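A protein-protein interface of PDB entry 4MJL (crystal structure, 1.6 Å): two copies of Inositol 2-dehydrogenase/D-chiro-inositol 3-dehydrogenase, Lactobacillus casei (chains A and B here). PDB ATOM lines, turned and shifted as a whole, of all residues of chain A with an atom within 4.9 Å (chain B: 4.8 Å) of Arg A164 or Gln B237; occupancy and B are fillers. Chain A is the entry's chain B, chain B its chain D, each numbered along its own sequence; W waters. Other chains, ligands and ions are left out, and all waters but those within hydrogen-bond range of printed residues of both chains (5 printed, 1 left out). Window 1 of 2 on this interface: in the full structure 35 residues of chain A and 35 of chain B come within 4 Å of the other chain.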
ATOM      1  N   VAL A 162      19.268  21.390  -4.682  1.00  0.00           N
ATOM      2  CA  VAL A 162      18.030  21.820  -3.996  1.00  0.00           C
ATOM      3  C   VAL A 162      18.369  21.956  -2.517  1.00  0.00           C
ATOM      4  O   VAL A 162      19.120  21.149  -1.963  1.00  0.00           O
ATOM      5  CB  VAL A 162      16.837  20.795  -4.197  1.00  0.00           C
ATOM      6  CG1 VAL A 162      15.569  21.248  -3.439  1.00  0.00           C
ATOM      7  CG2 VAL A 162      16.462  20.663  -5.644  1.00  0.00           C
ATOM      8  N   VAL A 163      17.838  22.989  -1.867  1.00  0.00           N
ATOM      9  CA  VAL A 163      17.909  23.079  -0.398  1.00  0.00           C
ATOM     10  C   VAL A 163      16.466  23.104   0.119  1.00  0.00           C
ATOM     11  O   VAL A 163      15.633  23.838  -0.434  1.00  0.00           O
ATOM     12  CB  VAL A 163      18.637  24.377   0.045  1.00  0.00           C
ATOM     13  CG1 VAL A 163      18.618  24.511   1.540  1.00  0.00           C
ATOM     14  CG2 VAL A 163      20.054  24.351  -0.471  1.00  0.00           C
ATOM     15  N   ARG A 164      16.152  22.291   1.115  1.00  0.00           N
ATOM     16  CA  ARG A 164      14.835  22.331   1.720  1.00  0.00           C
ATOM     17  C   ARG A 164      15.055  22.706   3.149  1.00  0.00           C
ATOM     18  O   ARG A 164      15.842  22.080   3.826  1.00  0.00           O
ATOM     19  CB  ARG A 164      14.152  20.999   1.657  1.00  0.00           C
ATOM     20  CG  ARG A 164      14.032  20.513   0.255  1.00  0.00           C
ATOM     21  CD  ARG A 164      13.129  19.254   0.205  1.00  0.00           C
ATOM     22  NE  ARG A 164      12.032  19.613  -0.642  1.00  0.00           N
ATOM     23  CZ  ARG A 164      11.005  18.850  -0.932  1.00  0.00           C
ATOM     24  NH1 ARG A 164      10.903  17.653  -0.427  1.00  0.00           N
ATOM     25  NH2 ARG A 164      10.113  19.312  -1.784  1.00  0.00           N
ATOM     26  N   ALA A 165      14.355  23.727   3.632  1.00  0.00           N
ATOM     27  CA  ALA A 165      14.619  24.249   4.969  1.00  0.00           C
ATOM     28  C   ALA A 165      13.292  24.564   5.652  1.00  0.00           C
ATOM     29  O   ALA A 165      12.292  24.751   4.962  1.00  0.00           O
ATOM     30  CB  ALA A 165      15.483  25.479   4.871  1.00  0.00           C
ATOM     31  N   SER A 166      13.278  24.554   6.976  1.00  0.00           N
ATOM     32  CA  SER A 166      12.101  24.949   7.757  1.00  0.00           C
ATOM     33  C   SER A 166      12.552  25.915   8.846  1.00  0.00           C
ATOM     34  O   SER A 166      13.600  25.723   9.461  1.00  0.00           O
ATOM     35  CB  SER A 166      11.409  23.771   8.431  1.00  0.00           C
ATOM     36  OG  SER A 166      10.915  22.848   7.452  1.00  0.00           O
ATOM     37  N   LEU A 225       5.384  29.815   2.176  1.00  0.00           N
ATOM     38  CA  LEU A 225       6.439  29.056   1.499  1.00  0.00           C
ATOM     39  C   LEU A 225       7.291  30.022   0.729  1.00  0.00           C
ATOM     40  O   LEU A 225       6.771  30.777  -0.078  1.00  0.00           O
ATOM     41  CB  LEU A 225       5.835  28.019   0.545  1.00  0.00           C
ATOM     42  CG  LEU A 225       5.004  26.989   1.263  1.00  0.00           C
ATOM     43  CD1 LEU A 225       4.194  26.159   0.236  1.00  0.00           C
ATOM     44  CD2 LEU A 225       5.921  26.102   2.014  1.00  0.00           C
ATOM     45  N   THR A 227      10.326  30.469  -1.991  1.00  0.00           N
ATOM     46  CA  THR A 227      11.179  29.789  -2.975  1.00  0.00           C
ATOM     47  C   THR A 227      12.217  30.772  -3.524  1.00  0.00           C
ATOM     48  O   THR A 227      11.859  31.836  -4.042  1.00  0.00           O
ATOM     49  CB  THR A 227      10.326  29.125  -4.103  1.00  0.00           C
ATOM     50  OG1 THR A 227       9.412  28.206  -3.490  1.00  0.00           O
ATOM     51  CG2 THR A 227      11.240  28.398  -5.087  1.00  0.00           C
ATOM     52  N   GLN A 237      13.808  25.945  -1.016  1.00  0.00           N
ATOM     53  CA  GLN A 237      12.413  25.918  -0.595  1.00  0.00           C
ATOM     54  C   GLN A 237      12.371  26.013   0.928  1.00  0.00           C
ATOM     55  O   GLN A 237      12.787  25.090   1.612  1.00  0.00           O
ATOM     56  CB  GLN A 237      11.746  24.625  -1.056  1.00  0.00           C
ATOM     57  CG  GLN A 237      11.742  24.419  -2.559  1.00  0.00           C
ATOM     58  CD  GLN A 237      11.015  23.164  -2.940  1.00  0.00           C
ATOM     59  OE1 GLN A 237      11.187  22.137  -2.290  1.00  0.00           O
ATOM     60  NE2 GLN A 237      10.151  23.239  -3.924  1.00  0.00           N
ATOM     61  N   LYS A 251      15.337  23.532  10.483  1.00  0.00           N
ATOM     62  CA  LYS A 251      15.641  22.325   9.686  1.00  0.00           C
ATOM     63  C   LYS A 251      16.317  22.737   8.410  1.00  0.00           C
ATOM     64  O   LYS A 251      16.015  23.784   7.858  1.00  0.00           O
ATOM     65  CB  LYS A 251      14.388  21.511   9.352  1.00  0.00           C
ATOM     66  CG  LYS A 251      13.524  21.072  10.584  1.00  0.00           C
ATOM     67  CD  LYS A 251      12.434  20.112  10.151  1.00  0.00           C
ATOM     68  CE  LYS A 251      11.278  20.083  11.172  1.00  0.00           C
ATOM     69  NZ  LYS A 251      10.339  19.118  10.634  1.00  0.00           N
ATOM     70  N   LEU A 252      17.273  21.925   7.954  1.00  0.00           N
ATOM     71  CA  LEU A 252      18.057  22.247   6.767  1.00  0.00           C
ATOM     72  C   LEU A 252      18.529  20.970   6.107  1.00  0.00           C
ATOM     73  O   LEU A 252      19.158  20.153   6.770  1.00  0.00           O
ATOM     74  CB  LEU A 252      19.306  23.051   7.141  1.00  0.00           C
ATOM     75  CG  LEU A 252      20.259  23.436   6.004  1.00  0.00           C
ATOM     76  CD1 LEU A 252      19.573  24.318   4.972  1.00  0.00           C
ATOM     77  CD2 LEU A 252      21.452  24.158   6.602  1.00  0.00           C
ATOM     78  N   GLU A 253      18.185  20.802   4.833  1.00  0.00           N
ATOM     79  CA  GLU A 253      18.589  19.626   4.081  1.00  0.00           C
ATOM     80  C   GLU A 253      19.123  20.119   2.761  1.00  0.00           C
ATOM     81  O   GLU A 253      18.503  20.941   2.091  1.00  0.00           O
ATOM     82  CB  GLU A 253      17.368  18.746   3.839  1.00  0.00           C
ATOM     83  CG  GLU A 253      17.605  17.519   2.940  1.00  0.00           C
ATOM     84  CD  GLU A 253      16.264  16.796   2.595  1.00  0.00           C
ATOM     85  OE1 GLU A 253      15.169  17.383   2.791  1.00  0.00           O
ATOM     86  OE2 GLU A 253      16.310  15.648   2.127  1.00  0.00           O
ATOM     87  N   VAL B 163       2.516  19.560   2.675  1.00  0.00           N
ATOM     88  CA  VAL B 163       3.061  18.210   2.636  1.00  0.00           C
ATOM     89  C   VAL B 163       4.386  18.352   1.921  1.00  0.00           C
ATOM     90  O   VAL B 163       4.499  19.028   0.926  1.00  0.00           O
ATOM     91  CB  VAL B 163       2.172  17.193   1.895  1.00  0.00           C
ATOM     92  CG1 VAL B 163       2.894  15.808   1.865  1.00  0.00           C
ATOM     93  CG2 VAL B 163       0.841  17.042   2.569  1.00  0.00           C
ATOM     94  N   ARG B 164       5.435  17.766   2.503  1.00  0.00           N
ATOM     95  CA  ARG B 164       6.723  17.716   1.835  1.00  0.00           C
ATOM     96  C   ARG B 164       7.089  16.275   1.614  1.00  0.00           C
ATOM     97  O   ARG B 164       7.021  15.450   2.536  1.00  0.00           O
ATOM     98  CB  ARG B 164       7.816  18.442   2.623  1.00  0.00           C
ATOM     99  CG  ARG B 164       7.492  19.905   2.742  1.00  0.00           C
ATOM    100  CD  ARG B 164       8.598  20.664   3.410  1.00  0.00           C
ATOM    101  NE  ARG B 164       8.959  21.816   2.589  1.00  0.00           N
ATOM    102  CZ  ARG B 164       9.936  22.657   2.906  1.00  0.00           C
ATOM    103  NH1 ARG B 164      10.622  22.456   4.027  1.00  0.00           N
ATOM    104  NH2 ARG B 164      10.190  23.688   2.132  1.00  0.00           N
ATOM    105  N   ALA B 165       7.471  15.966   0.374  1.00  0.00           N
ATOM    106  CA  ALA B 165       7.734  14.576   0.050  1.00  0.00           C
ATOM    107  C   ALA B 165       8.978  14.499  -0.830  1.00  0.00           C
ATOM    108  O   ALA B 165       9.278  15.425  -1.551  1.00  0.00           O
ATOM    109  CB  ALA B 165       6.524  13.919  -0.662  1.00  0.00           C
ATOM    110  N   SER B 166       9.690  13.365  -0.743  1.00  0.00           N
ATOM    111  CA  SER B 166      10.797  13.069  -1.658  1.00  0.00           C
ATOM    112  C   SER B 166      10.601  11.693  -2.276  1.00  0.00           C
ATOM    113  O   SER B 166      10.203  10.741  -1.608  1.00  0.00           O
ATOM    114  CB  SER B 166      12.176  13.060  -0.931  1.00  0.00           C
ATOM    115  OG  SER B 166      12.473  14.319  -0.370  1.00  0.00           O
ATOM    116  N   LEU B 225      11.119  19.433  -9.338  1.00  0.00           N
ATOM    117  CA  LEU B 225      10.301  19.821  -8.199  1.00  0.00           C
ATOM    118  C   LEU B 225       8.856  19.931  -8.670  1.00  0.00           C
ATOM    119  O   LEU B 225       8.594  20.602  -9.662  1.00  0.00           O
ATOM    120  CB  LEU B 225      10.770  21.164  -7.625  1.00  0.00           C
ATOM    121  CG  LEU B 225      12.218  21.199  -7.113  1.00  0.00           C
ATOM    122  CD1 LEU B 225      12.712  22.640  -6.810  1.00  0.00           C
ATOM    123  CD2 LEU B 225      12.328  20.348  -5.854  1.00  0.00           C
ATOM    124  N   ALA B 226       7.951  19.284  -7.964  1.00  0.00           N
ATOM    125  CA  ALA B 226       6.537  19.357  -8.283  1.00  0.00           C
ATOM    126  C   ALA B 226       5.792  20.051  -7.156  1.00  0.00           C
ATOM    127  O   ALA B 226       5.922  19.675  -6.017  1.00  0.00           O
ATOM    128  CB  ALA B 226       5.977  17.959  -8.496  1.00  0.00           C
ATOM    129  N   THR B 227       4.994  21.067  -7.470  1.00  0.00           N
ATOM    130  CA  THR B 227       4.123  21.669  -6.465  1.00  0.00           C
ATOM    131  C   THR B 227       2.692  21.406  -6.852  1.00  0.00           C
ATOM    132  O   THR B 227       2.273  21.774  -7.933  1.00  0.00           O
ATOM    133  CB  THR B 227       4.297  23.161  -6.412  1.00  0.00           C
ATOM    134  OG1 THR B 227       5.650  23.481  -6.035  1.00  0.00           O
ATOM    135  CG2 THR B 227       3.364  23.754  -5.356  1.00  0.00           C
ATOM    136  N   VAL B 235      -0.751  22.618   0.214  1.00  0.00           N
ATOM    137  CA  VAL B 235       0.263  22.650  -0.831  1.00  0.00           C
ATOM    138  C   VAL B 235       1.214  21.489  -0.611  1.00  0.00           C
ATOM    139  O   VAL B 235       1.718  21.291   0.495  1.00  0.00           O
ATOM    140  CB  VAL B 235       1.055  23.975  -0.838  1.00  0.00           C
ATOM    141  CG1 VAL B 235       2.166  23.966  -1.847  1.00  0.00           C
ATOM    142  CG2 VAL B 235       0.099  25.166  -1.144  1.00  0.00           C
ATOM    143  N   ILE B 236       1.427  20.739  -1.669  1.00  0.00           N
ATOM    144  CA  ILE B 236       2.362  19.605  -1.627  1.00  0.00           C
ATOM    145  C   ILE B 236       3.611  19.933  -2.437  1.00  0.00           C
ATOM    146  O   ILE B 236       3.512  20.305  -3.583  1.00  0.00           O
ATOM    147  CB  ILE B 236       1.683  18.342  -2.176  1.00  0.00           C
ATOM    148  CG1 ILE B 236       0.409  18.061  -1.372  1.00  0.00           C
ATOM    149  CG2 ILE B 236       2.702  17.174  -2.178  1.00  0.00           C
ATOM    150  CD1 ILE B 236      -0.724  17.833  -2.261  1.00  0.00           C
ATOM    151  N   GLN B 237       4.780  19.794  -1.820  1.00  0.00           N
ATOM    152  CA  GLN B 237       6.033  19.992  -2.545  1.00  0.00           C
ATOM    153  C   GLN B 237       6.780  18.661  -2.610  1.00  0.00           C
ATOM    154  O   GLN B 237       7.262  18.190  -1.580  1.00  0.00           O
ATOM    155  CB  GLN B 237       6.940  20.990  -1.803  1.00  0.00           C
ATOM    156  CG  GLN B 237       6.312  22.388  -1.627  1.00  0.00           C
ATOM    157  CD  GLN B 237       7.265  23.364  -0.903  1.00  0.00           C
ATOM    158  OE1 GLN B 237       7.891  23.018   0.105  1.00  0.00           O
ATOM    159  NE2 GLN B 237       7.386  24.572  -1.433  1.00  0.00           N
ATOM    160  N   VAL B 238       6.915  18.105  -3.806  1.00  0.00           N
ATOM    161  CA  VAL B 238       7.613  16.834  -4.017  1.00  0.00           C
ATOM    162  C   VAL B 238       8.929  17.089  -4.685  1.00  0.00           C
ATOM    163  O   VAL B 238       9.009  17.799  -5.668  1.00  0.00           O
ATOM    164  CB  VAL B 238       6.782  15.878  -4.918  1.00  0.00           C
ATOM    165  CG1 VAL B 238       7.465  14.482  -4.923  1.00  0.00           C
ATOM    166  CG2 VAL B 238       5.343  15.781  -4.382  1.00  0.00           C
ATOM    167  N   LEU B 239       9.964  16.470  -4.147  1.00  0.00           N
ATOM    168  CA  LEU B 239      11.255  16.427  -4.798  1.00  0.00           C
ATOM    169  C   LEU B 239      11.342  15.080  -5.511  1.00  0.00           C
ATOM    170  O   LEU B 239      11.211  14.056  -4.886  1.00  0.00           O
ATOM    171  CB  LEU B 239      12.392  16.483  -3.761  1.00  0.00           C
ATOM    172  CG  LEU B 239      13.789  16.099  -4.301  1.00  0.00           C
ATOM    173  CD1 LEU B 239      14.257  17.157  -5.316  1.00  0.00           C
ATOM    174  CD2 LEU B 239      14.724  15.965  -3.165  1.00  0.00           C
HETATM  175  O   HOH W   1      10.856  20.112   5.756  1.00  0.00           O
HETATM  176  O   HOH W   2       8.590  20.741  -4.640  1.00  0.00           O
HETATM  177  O   HOH W   3       9.074  26.676  -0.427  1.00  0.00           O
HETATM  178  O   HOH W   4      15.128  14.362   0.166  1.00  0.00           O
HETATM  179  O   HOH W   5      12.709  16.792   1.739  1.00  0.00           O
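The guanidinium group (NH1) of Arg A164 is in hydrogen-bond range of the backbone carbonyl oxygen (O) of Ala B165 (3.0 Å). NH2 of Arg A164 is in hydrogen-bond range of O of Gln B237, 3.1 Å away. The backbone carbonyl oxygen (O) of Ala A165 lies within hydrogen-bond range of the guanidinium group (NH1) of Arg B164 (3.0 Å). OG of Ser A166 lies within hydrogen-bond range of NH1 of Arg B164 (3.5 Å). O of Gln A237 lies within hydrogen-bond range of NH2 of Arg B164 (3.0 Å).
N of Gln A237 sits at hydrogen-bond distance from O of Val A163. The side-chain amide oxygen (OE1) of Gln A237 sits at hydrogen-bond distance from the guanidinium group (NH2) of Arg A164, at 3.1 Å. O of Arg A164 is in hydrogen-bond range of N of Glu A253, 2.9 Å away. The backbone NH (N) of Val B163 lies within hydrogen-bond range of the backbone carbonyl oxygen (O) of Val B235. The backbone carbonyl oxygen (O) of Gln B237 lies within hydrogen-bond range of the backbone NH (N) of Ala B165, 3.0 Å away. The backbone NH (N) of Leu B239 sits at hydrogen-bond distance from the backbone carbonyl oxygen (O) of Ala B165.
Arg A164 touches Ser B166 (NH1 to OG, 3.7 Å). NH2 of Arg A164 touches C of Val B238, at 3.8 Å. NH2 of Arg A164 touches N of Leu B239, 3.7 Å away. CG1 of Val B235 touches CD1 of Leu A225 (3.6 Å). Gln B237 touches Leu A225. Gln A237 touches Leu B225. NE2 of Gln A237 touches NE2 of Gln B237, at 3.95 Å.
Arg A164 touches just these residues of chain B: Ala B165 (3.0 Å), Ser B166 (3.7 Å), Gln B237 (3.1 Å), Val B238 (3.8 Å) and Leu B239 (3.7 Å). Gln B237 touches just these residues of chain A: Arg A164, Leu A225 and Gln A237. Printed residues of chain B within 4 Å of Gln A237: Arg B164, Leu B225 and Gln B237. Of the printed residues of chain B, Ala A165 touches Arg B164. Of the printed residues of chain A, Ala B165 touches Arg A164. Printed residues of chain A within 4 Å of Leu B225: Gln A237 (3.9 Å). Glu A253 touches none of the printed residues of chain B. The nearest residue of chain B that does not touch Arg A164 is Arg B164 (4.4 Å). The nearest printed residue of chain A that does not touch Arg B164 is Arg A164 (4.4 Å).
Hydrophobic or aromatic side chains of chain A within 4 Å of the printed part of chain B: Leu A225. Along chain A the printed residues that touch a printed residue of chain B span positions 164 to 237. Hydrophobic or aromatic side chains of chain B that line the printed part of chain A: Leu B225, Val B235 and Leu B239. Among the printed residues, no Asp or Glu carboxylate lies within 4 Å of a Lys or Arg side-chain nitrogen of the other chain.
Arg A164 touches Ala B165, and with the chains exchanged Ala A165 touches Arg B164. Arg A164 touches Ser B166, and with the chains exchanged Ser A166 touches Arg B164. Leu A225 touches Gln B237, and with the chains exchanged Gln A237 touches Leu B225. Gln B237 touches its own counterpart, Gln A237. 7 positions are printed for both chains. Of the 12 pairs that touch across the chains among the printed residues, 9 have their exchanged pair printed and touching as well.
Water W4 lies within hydrogen-bond range of OE2 of Glu A253 and OG of Ser B166. Water W5 lies within hydrogen-bond range of the side-chain carboxylate of Glu A253, the guanidinium group of Arg A164 and the side-chain hydroxyl of Ser B166. Water W3 lies within hydrogen-bond range of NE2 of Gln B237 (2.9 Å) and OG1 of Thr A227 (3.4 Å). Water W1 bridges NH1 of Arg B164 and OG of Ser A166. Water W2 lies within hydrogen-bond range of the side-chain amide nitrogen of Gln A237 (3.0 Å), the backbone carbonyl oxygen of Val B238 (3.1 Å) and the backbone carbonyl oxygen of Ala B226 (3.2 Å).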
